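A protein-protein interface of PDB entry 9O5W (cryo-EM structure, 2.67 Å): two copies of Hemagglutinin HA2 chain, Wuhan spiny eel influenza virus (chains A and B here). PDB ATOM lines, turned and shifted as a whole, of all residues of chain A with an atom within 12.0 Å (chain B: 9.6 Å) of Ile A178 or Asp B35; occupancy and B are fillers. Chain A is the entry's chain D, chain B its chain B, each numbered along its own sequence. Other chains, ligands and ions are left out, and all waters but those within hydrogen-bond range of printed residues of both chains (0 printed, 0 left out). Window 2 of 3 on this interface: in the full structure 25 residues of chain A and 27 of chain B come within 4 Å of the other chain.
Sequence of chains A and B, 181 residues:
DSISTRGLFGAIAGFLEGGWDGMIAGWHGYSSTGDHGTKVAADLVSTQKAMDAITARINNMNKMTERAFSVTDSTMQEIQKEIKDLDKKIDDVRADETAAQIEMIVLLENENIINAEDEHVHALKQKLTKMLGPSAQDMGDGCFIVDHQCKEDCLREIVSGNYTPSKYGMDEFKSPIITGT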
ATOM      1  N   PHE A 173     -11.190  -8.199  21.922  1.00  0.00           N
ATOM      2  CA  PHE A 173     -11.577  -6.853  21.557  1.00  0.00           C
ATOM      3  C   PHE A 173     -10.768  -6.414  20.345  1.00  0.00           C
ATOM      4  O   PHE A 173      -9.615  -6.816  20.163  1.00  0.00           O
ATOM      5  CB  PHE A 173     -11.334  -5.916  22.736  1.00  0.00           C
ATOM      6  CG  PHE A 173     -12.333  -6.081  23.838  1.00  0.00           C
ATOM      7  CD1 PHE A 173     -13.596  -5.534  23.743  1.00  0.00           C
ATOM      8  CD2 PHE A 173     -12.009  -6.814  24.964  1.00  0.00           C
ATOM      9  CE1 PHE A 173     -14.510  -5.698  24.763  1.00  0.00           C
ATOM     10  CE2 PHE A 173     -12.916  -6.983  25.982  1.00  0.00           C
ATOM     11  CZ  PHE A 173     -14.170  -6.431  25.880  1.00  0.00           C
ATOM     12  N   LYS A 174     -11.386  -5.592  19.502  1.00  0.00           N
ATOM     13  CA  LYS A 174     -10.681  -5.078  18.338  1.00  0.00           C
ATOM     14  C   LYS A 174      -9.537  -4.200  18.820  1.00  0.00           C
ATOM     15  O   LYS A 174      -9.668  -3.474  19.808  1.00  0.00           O
ATOM     16  CB  LYS A 174     -11.622  -4.291  17.427  1.00  0.00           C
ATOM     17  CG  LYS A 174     -12.673  -5.144  16.735  1.00  0.00           C
ATOM     18  CD  LYS A 174     -13.572  -4.324  15.809  1.00  0.00           C
ATOM     19  CE  LYS A 174     -14.675  -3.565  16.542  1.00  0.00           C
ATOM     20  NZ  LYS A 174     -14.187  -2.325  17.210  1.00  0.00           N
ATOM     21  N   SER A 175      -8.403  -4.277  18.133  1.00  0.00           N
ATOM     22  CA  SER A 175      -7.284  -3.453  18.531  1.00  0.00           C
ATOM     23  C   SER A 175      -7.572  -1.984  18.217  1.00  0.00           C
ATOM     24  O   SER A 175      -8.408  -1.672  17.365  1.00  0.00           O
ATOM     25  CB  SER A 175      -6.017  -3.912  17.818  1.00  0.00           C
ATOM     26  OG  SER A 175      -6.093  -3.657  16.427  1.00  0.00           O
ATOM     27  N   PRO A 176      -6.879  -1.058  18.892  1.00  0.00           N
ATOM     28  CA  PRO A 176      -7.056   0.370  18.581  1.00  0.00           C
ATOM     29  C   PRO A 176      -6.405   0.827  17.291  1.00  0.00           C
ATOM     30  O   PRO A 176      -6.591   1.991  16.916  1.00  0.00           O
ATOM     31  CB  PRO A 176      -6.421   1.066  19.784  1.00  0.00           C
ATOM     32  CG  PRO A 176      -5.406   0.119  20.267  1.00  0.00           C
ATOM     33  CD  PRO A 176      -5.990  -1.243  20.055  1.00  0.00           C
ATOM     34  N   ILE A 177      -5.664  -0.029  16.602  1.00  0.00           N
ATOM     35  CA  ILE A 177      -4.935   0.372  15.405  1.00  0.00           C
ATOM     36  C   ILE A 177      -5.836   0.154  14.198  1.00  0.00           C
ATOM     37  O   ILE A 177      -6.350  -0.948  13.980  1.00  0.00           O
ATOM     38  CB  ILE A 177      -3.623  -0.423  15.269  1.00  0.00           C
ATOM     39  CG1 ILE A 177      -2.749  -0.369  16.544  1.00  0.00           C
ATOM     40  CG2 ILE A 177      -2.792   0.099  14.089  1.00  0.00           C
ATOM     41  CD1 ILE A 177      -2.787   0.920  17.392  1.00  0.00           C
ATOM     42  N   ILE A 178      -6.025   1.214  13.418  1.00  0.00           N
ATOM     43  CA  ILE A 178      -6.917   1.204  12.267  1.00  0.00           C
ATOM     44  C   ILE A 178      -6.540   2.349  11.331  1.00  0.00           C
ATOM     45  O   ILE A 178      -6.598   2.211  10.109  1.00  0.00           O
ATOM     46  CB  ILE A 178      -8.407   1.292  12.702  1.00  0.00           C
ATOM     47  CG1 ILE A 178      -9.321   1.140  11.478  1.00  0.00           C
ATOM     48  CG2 ILE A 178      -8.690   2.592  13.480  1.00  0.00           C
ATOM     49  CD1 ILE A 178     -10.786   0.898  11.803  1.00  0.00           C
ATOM     50  N   SER B  32      -7.262   9.165  23.883  1.00  0.00           N
ATOM     51  CA  SER B  32      -7.412   8.317  22.703  1.00  0.00           C
ATOM     52  C   SER B  32      -6.039   7.785  22.325  1.00  0.00           C
ATOM     53  O   SER B  32      -5.159   8.567  21.954  1.00  0.00           O
ATOM     54  CB  SER B  32      -8.027   9.098  21.539  1.00  0.00           C
ATOM     55  OG  SER B  32      -8.068   8.309  20.365  1.00  0.00           O
ATOM     56  N   THR B  33      -5.857   6.466  22.406  1.00  0.00           N
ATOM     57  CA  THR B  33      -4.577   5.824  22.108  1.00  0.00           C
ATOM     58  C   THR B  33      -4.706   4.902  20.903  1.00  0.00           C
ATOM     59  O   THR B  33      -5.496   3.953  20.925  1.00  0.00           O
ATOM     60  CB  THR B  33      -4.049   5.038  23.317  1.00  0.00           C
ATOM     61  OG1 THR B  33      -2.961   4.202  22.902  1.00  0.00           O
ATOM     62  CG2 THR B  33      -5.123   4.169  23.966  1.00  0.00           C
ATOM     63  N   GLY B  34      -3.936   5.183  19.848  1.00  0.00           N
ATOM     64  CA  GLY B  34      -4.021   4.374  18.643  1.00  0.00           C
ATOM     65  C   GLY B  34      -2.889   4.569  17.650  1.00  0.00           C
ATOM     66  O   GLY B  34      -1.729   4.748  18.039  1.00  0.00           O
ATOM     67  N   ASP B  35      -3.241   4.641  16.360  1.00  0.00           N
ATOM     68  CA  ASP B  35      -2.248   4.771  15.294  1.00  0.00           C
ATOM     69  C   ASP B  35      -1.485   6.086  15.386  1.00  0.00           C
ATOM     70  O   ASP B  35      -0.374   6.192  14.859  1.00  0.00           O
ATOM     71  CB  ASP B  35      -2.925   4.614  13.925  1.00  0.00           C
ATOM     72  CG  ASP B  35      -3.974   5.692  13.636  1.00  0.00           C
ATOM     73  OD1 ASP B  35      -3.703   6.901  13.786  1.00  0.00           O
ATOM     74  OD2 ASP B  35      -5.100   5.312  13.249  1.00  0.00           O
ATOM     75  N   HIS B  36      -2.071   7.073  16.051  1.00  0.00           N
ATOM     76  CA  HIS B  36      -1.551   8.421  16.192  1.00  0.00           C
ATOM     77  C   HIS B  36      -0.923   8.615  17.564  1.00  0.00           C
ATOM     78  O   HIS B  36      -0.658   9.753  17.961  1.00  0.00           O
ATOM     79  CB  HIS B  36      -2.667   9.456  15.982  1.00  0.00           C
ATOM     80  CG  HIS B  36      -3.869   9.252  16.860  1.00  0.00           C
ATOM     81  ND1 HIS B  36      -4.108  10.019  17.977  1.00  0.00           N
ATOM     82  CD2 HIS B  36      -4.901   8.376  16.782  1.00  0.00           C
ATOM     83  CE1 HIS B  36      -5.226   9.618  18.557  1.00  0.00           C
ATOM     84  NE2 HIS B  36      -5.728   8.624  17.849  1.00  0.00           N
ATOM     85  N   GLY B  37      -0.682   7.523  18.295  1.00  0.00           N
ATOM     86  CA  GLY B  37      -0.150   7.636  19.636  1.00  0.00           C
ATOM     87  C   GLY B  37      -1.283   7.996  20.579  1.00  0.00           C
ATOM     88  O   GLY B  37      -2.444   7.671  20.322  1.00  0.00           O
ATOM     89  N   THR B  38      -0.940   8.633  21.697  1.00  0.00           N
ATOM     90  CA  THR B  38      -1.916   8.977  22.721  1.00  0.00           C
ATOM     91  C   THR B  38      -2.198  10.474  22.721  1.00  0.00           C
ATOM     92  O   THR B  38      -1.274  11.284  22.853  1.00  0.00           O
ATOM     93  CB  THR B  38      -1.405   8.540  24.101  1.00  0.00           C
ATOM     94  OG1 THR B  38      -1.188   7.126  24.104  1.00  0.00           O
ATOM     95  CG2 THR B  38      -2.413   8.868  25.213  1.00  0.00           C
ATOM     96  N   LYS B  39      -3.472  10.829  22.576  1.00  0.00           N
ATOM     97  CA  LYS B  39      -3.955  12.201  22.637  1.00  0.00           C
ATOM     98  C   LYS B  39      -4.772  12.318  23.911  1.00  0.00           C
ATOM     99  O   LYS B  39      -5.413  11.351  24.328  1.00  0.00           O
ATOM    100  CB  LYS B  39      -4.806  12.578  21.420  1.00  0.00           C
ATOM    101  CG  LYS B  39      -4.128  12.428  20.069  1.00  0.00           C
ATOM    102  CD  LYS B  39      -2.921  13.351  19.870  1.00  0.00           C
ATOM    103  CE  LYS B  39      -1.831  12.694  19.039  1.00  0.00           C
ATOM    104  NZ  LYS B  39      -0.838  11.983  19.888  1.00  0.00           N
ATOM    105  N   ILE B 145     -13.635   0.684  22.291  1.00  0.00           N
ATOM    106  CA  ILE B 145     -13.022   0.571  20.972  1.00  0.00           C
ATOM    107  C   ILE B 145     -14.037   0.978  19.913  1.00  0.00           C
ATOM    108  O   ILE B 145     -15.154   0.451  19.880  1.00  0.00           O
ATOM    109  CB  ILE B 145     -12.507  -0.857  20.711  1.00  0.00           C
ATOM    110  CG1 ILE B 145     -11.572  -1.339  21.834  1.00  0.00           C
ATOM    111  CG2 ILE B 145     -11.802  -0.952  19.350  1.00  0.00           C
ATOM    112  CD1 ILE B 145     -10.295  -0.535  22.022  1.00  0.00           C
ATOM    113  N   VAL B 146     -13.642   1.915  19.051  1.00  0.00           N
ATOM    114  CA  VAL B 146     -14.473   2.425  17.969  1.00  0.00           C
ATOM    115  C   VAL B 146     -13.704   2.222  16.669  1.00  0.00           C
ATOM    116  O   VAL B 146     -12.482   2.395  16.643  1.00  0.00           O
ATOM    117  CB  VAL B 146     -14.846   3.905  18.200  1.00  0.00           C
ATOM    118  CG1 VAL B 146     -15.653   4.046  19.477  1.00  0.00           C
ATOM    119  CG2 VAL B 146     -13.594   4.783  18.299  1.00  0.00           C
ATOM    120  N   ASP B 147     -14.409   1.869  15.593  1.00  0.00           N
ATOM    121  CA  ASP B 147     -13.742   1.599  14.316  1.00  0.00           C
ATOM    122  C   ASP B 147     -13.567   2.885  13.497  1.00  0.00           C
ATOM    123  O   ASP B 147     -14.069   3.031  12.382  1.00  0.00           O
ATOM    124  CB  ASP B 147     -14.529   0.542  13.540  1.00  0.00           C
ATOM    125  CG  ASP B 147     -14.088  -0.891  13.848  1.00  0.00           C
ATOM    126  OD1 ASP B 147     -12.962  -1.117  14.342  1.00  0.00           O
ATOM    127  OD2 ASP B 147     -14.898  -1.809  13.599  1.00  0.00           O
ATOM    128  N   HIS B 148     -12.842   3.838  14.071  1.00  0.00           N
ATOM    129  CA  HIS B 148     -12.518   5.070  13.364  1.00  0.00           C
ATOM    130  C   HIS B 148     -11.303   5.676  14.043  1.00  0.00           C
ATOM    131  O   HIS B 148     -10.949   5.294  15.162  1.00  0.00           O
ATOM    132  CB  HIS B 148     -13.683   6.063  13.323  1.00  0.00           C
ATOM    133  CG  HIS B 148     -14.019   6.663  14.647  1.00  0.00           C
ATOM    134  ND1 HIS B 148     -13.404   7.800  15.122  1.00  0.00           N
ATOM    135  CD2 HIS B 148     -14.926   6.305  15.585  1.00  0.00           C
ATOM    136  CE1 HIS B 148     -13.902   8.106  16.305  1.00  0.00           C
ATOM    137  NE2 HIS B 148     -14.828   7.216  16.608  1.00  0.00           N
ATOM    138  N   GLN B 149     -10.664   6.624  13.364  1.00  0.00           N
ATOM    139  CA  GLN B 149      -9.559   7.333  13.987  1.00  0.00           C
ATOM    140  C   GLN B 149     -10.166   8.435  14.849  1.00  0.00           C
ATOM    141  O   GLN B 149     -11.087   9.136  14.420  1.00  0.00           O
ATOM    142  CB  GLN B 149      -8.644   7.897  12.891  1.00  0.00           C
ATOM    143  CG  GLN B 149      -7.606   8.958  13.279  1.00  0.00           C
ATOM    144  CD  GLN B 149      -6.183   8.542  12.912  1.00  0.00           C
ATOM    145  OE1 GLN B 149      -5.950   7.881  11.899  1.00  0.00           O
ATOM    146  NE2 GLN B 149      -5.225   8.956  13.721  1.00  0.00           N
ATOM    147  N   CYS B 150      -9.648   8.586  16.067  1.00  0.00           N
ATOM    148  CA  CYS B 150     -10.116   9.586  17.032  1.00  0.00           C
ATOM    149  C   CYS B 150      -8.914  10.458  17.398  1.00  0.00           C
ATOM    150  O   CYS B 150      -8.181  10.122  18.331  1.00  0.00           O
ATOM    151  CB  CYS B 150     -10.732   8.820  18.233  1.00  0.00           C
ATOM    152  SG  CYS B 150     -11.564   9.664  19.623  1.00  0.00           S
ATOM    153  N   LYS B 151      -8.719  11.575  16.688  1.00  0.00           N
ATOM    154  CA  LYS B 151      -7.534  12.422  16.869  1.00  0.00           C
ATOM    155  C   LYS B 151      -7.907  13.853  17.267  1.00  0.00           C
ATOM    156  O   LYS B 151      -8.230  14.681  16.409  1.00  0.00           O
ATOM    157  CB  LYS B 151      -6.701  12.402  15.586  1.00  0.00           C
ATOM    158  CG  LYS B 151      -5.379  13.162  15.647  1.00  0.00           C
ATOM    159  CD  LYS B 151      -4.659  13.093  14.303  1.00  0.00           C
ATOM    160  CE  LYS B 151      -3.325  13.828  14.327  1.00  0.00           C
ATOM    161  NZ  LYS B 151      -2.631  13.765  13.009  1.00  0.00           N
ATOM    162  N   TYR B 168     -18.824   9.954  12.054  1.00  0.00           N
ATOM    163  CA  TYR B 168     -17.638   9.156  11.767  1.00  0.00           C
ATOM    164  C   TYR B 168     -17.963   7.850  11.052  1.00  0.00           C
ATOM    165  O   TYR B 168     -17.067   7.017  10.875  1.00  0.00           O
ATOM    166  CB  TYR B 168     -16.890   8.828  13.061  1.00  0.00           C
ATOM    167  CG  TYR B 168     -16.412  10.017  13.856  1.00  0.00           C
ATOM    168  CD1 TYR B 168     -15.200  10.626  13.569  1.00  0.00           C
ATOM    169  CD2 TYR B 168     -17.162  10.515  14.909  1.00  0.00           C
ATOM    170  CE1 TYR B 168     -14.756  11.707  14.298  1.00  0.00           C
ATOM    171  CE2 TYR B 168     -16.724  11.591  15.648  1.00  0.00           C
ATOM    172  CZ  TYR B 168     -15.516  12.178  15.343  1.00  0.00           C
ATOM    173  OH  TYR B 168     -15.081  13.257  16.078  1.00  0.00           O
ATOM    174  N   MET B 170     -20.194   5.567  12.211  1.00  0.00           N
ATOM    175  CA  MET B 170     -20.493   4.562  13.217  1.00  0.00           C
ATOM    176  C   MET B 170     -22.001   4.447  13.393  1.00  0.00           C
ATOM    177  O   MET B 170     -22.743   5.412  13.196  1.00  0.00           O
ATOM    178  CB  MET B 170     -19.836   4.918  14.553  1.00  0.00           C
ATOM    179  CG  MET B 170     -18.318   4.998  14.516  1.00  0.00           C
ATOM    180  SD  MET B 170     -17.538   3.391  14.274  1.00  0.00           S
ATOM    181  CE  MET B 170     -17.086   3.480  12.545  1.00  0.00           C
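Printed residues of chain A that touch a printed residue of chain B: Lys A174, Ser A175, Pro A176, Ile A177 and Ile A178.
Hydrophobic or aromatic side chains of chain A that line the printed part of chain B: Pro A176, Ile A177 and Ile A178.
Printed residues of chain B that touch a printed residue of chain A: Thr B33, Gly B34, Asp B35, Ile B145, Asp B147 and His B148.
Hydrophobic or aromatic side chains of chain B that line the printed part of chain A: Ile B145.
Of chain B, only Asp B35, Asp B147 and His B148 come within 4 Å of Ile A178.
Asp B35 touches two residues of chain A.
Of chain B, only Gly B34 (3.7 Å) and Asp B35 (3.9 Å) come within 4 Å of Ile A177.
Gly B34 touches two residues of chain A.
No residue of chain A comes within 4 Å of Gly B37.
Asp B147 touches just these residues of chain A: Lys A174 and Ile A178.
No residue of chain A comes within 4 Å of Gln B149.
Printed residues of chain A within 4 Å of Ile B145: Lys A174 (3.3 Å) and Ser A175 (3.997 Å).
Of the printed residues of chain B, Pro A176 touches Thr B33 and Gly B34.
Of the printed residues of chain B, Ser A175 touches Ile B145 (3.997 Å).
The nearest printed residue of chain B that does not touch Pro A176 is Asp B35 (4.3 Å).
OD1 of Asp B147 is in salt-bridge range of NZ of Lys A174 (3.3 Å).
Ile B145 touches Lys A174.
O of Ser A175 touches CG2 of Ile B145, 3.997 Å away.
O of Thr B33 touches CB of Pro A176, 3.2 Å away.
O of Pro A176 touches CA of Gly B34, at 3.9 Å.
C of Gly B34 touches CD1 of Ile A177, 3.7 Å away.
Asp B35 touches Ile A177.
Ile A178 touches Asp B35 (C to OD2, 3.8 Å).
C of Asp B147 touches CD1 of Ile A178, 3.8 Å away.
Ile A178 touches His B148 (CG2 to O, 3.9 Å).
The side-chain carboxylate (OD1) of Asp B35 is in hydrogen-bond range of the side-chain amide nitrogen (NE2) of Gln B149 (2.6 Å).
The backbone NH of Asp B147 lies within hydrogen-bond range of the side-chain sulfur of Met B170 (3.7 Å).
No position is printed for both chains.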
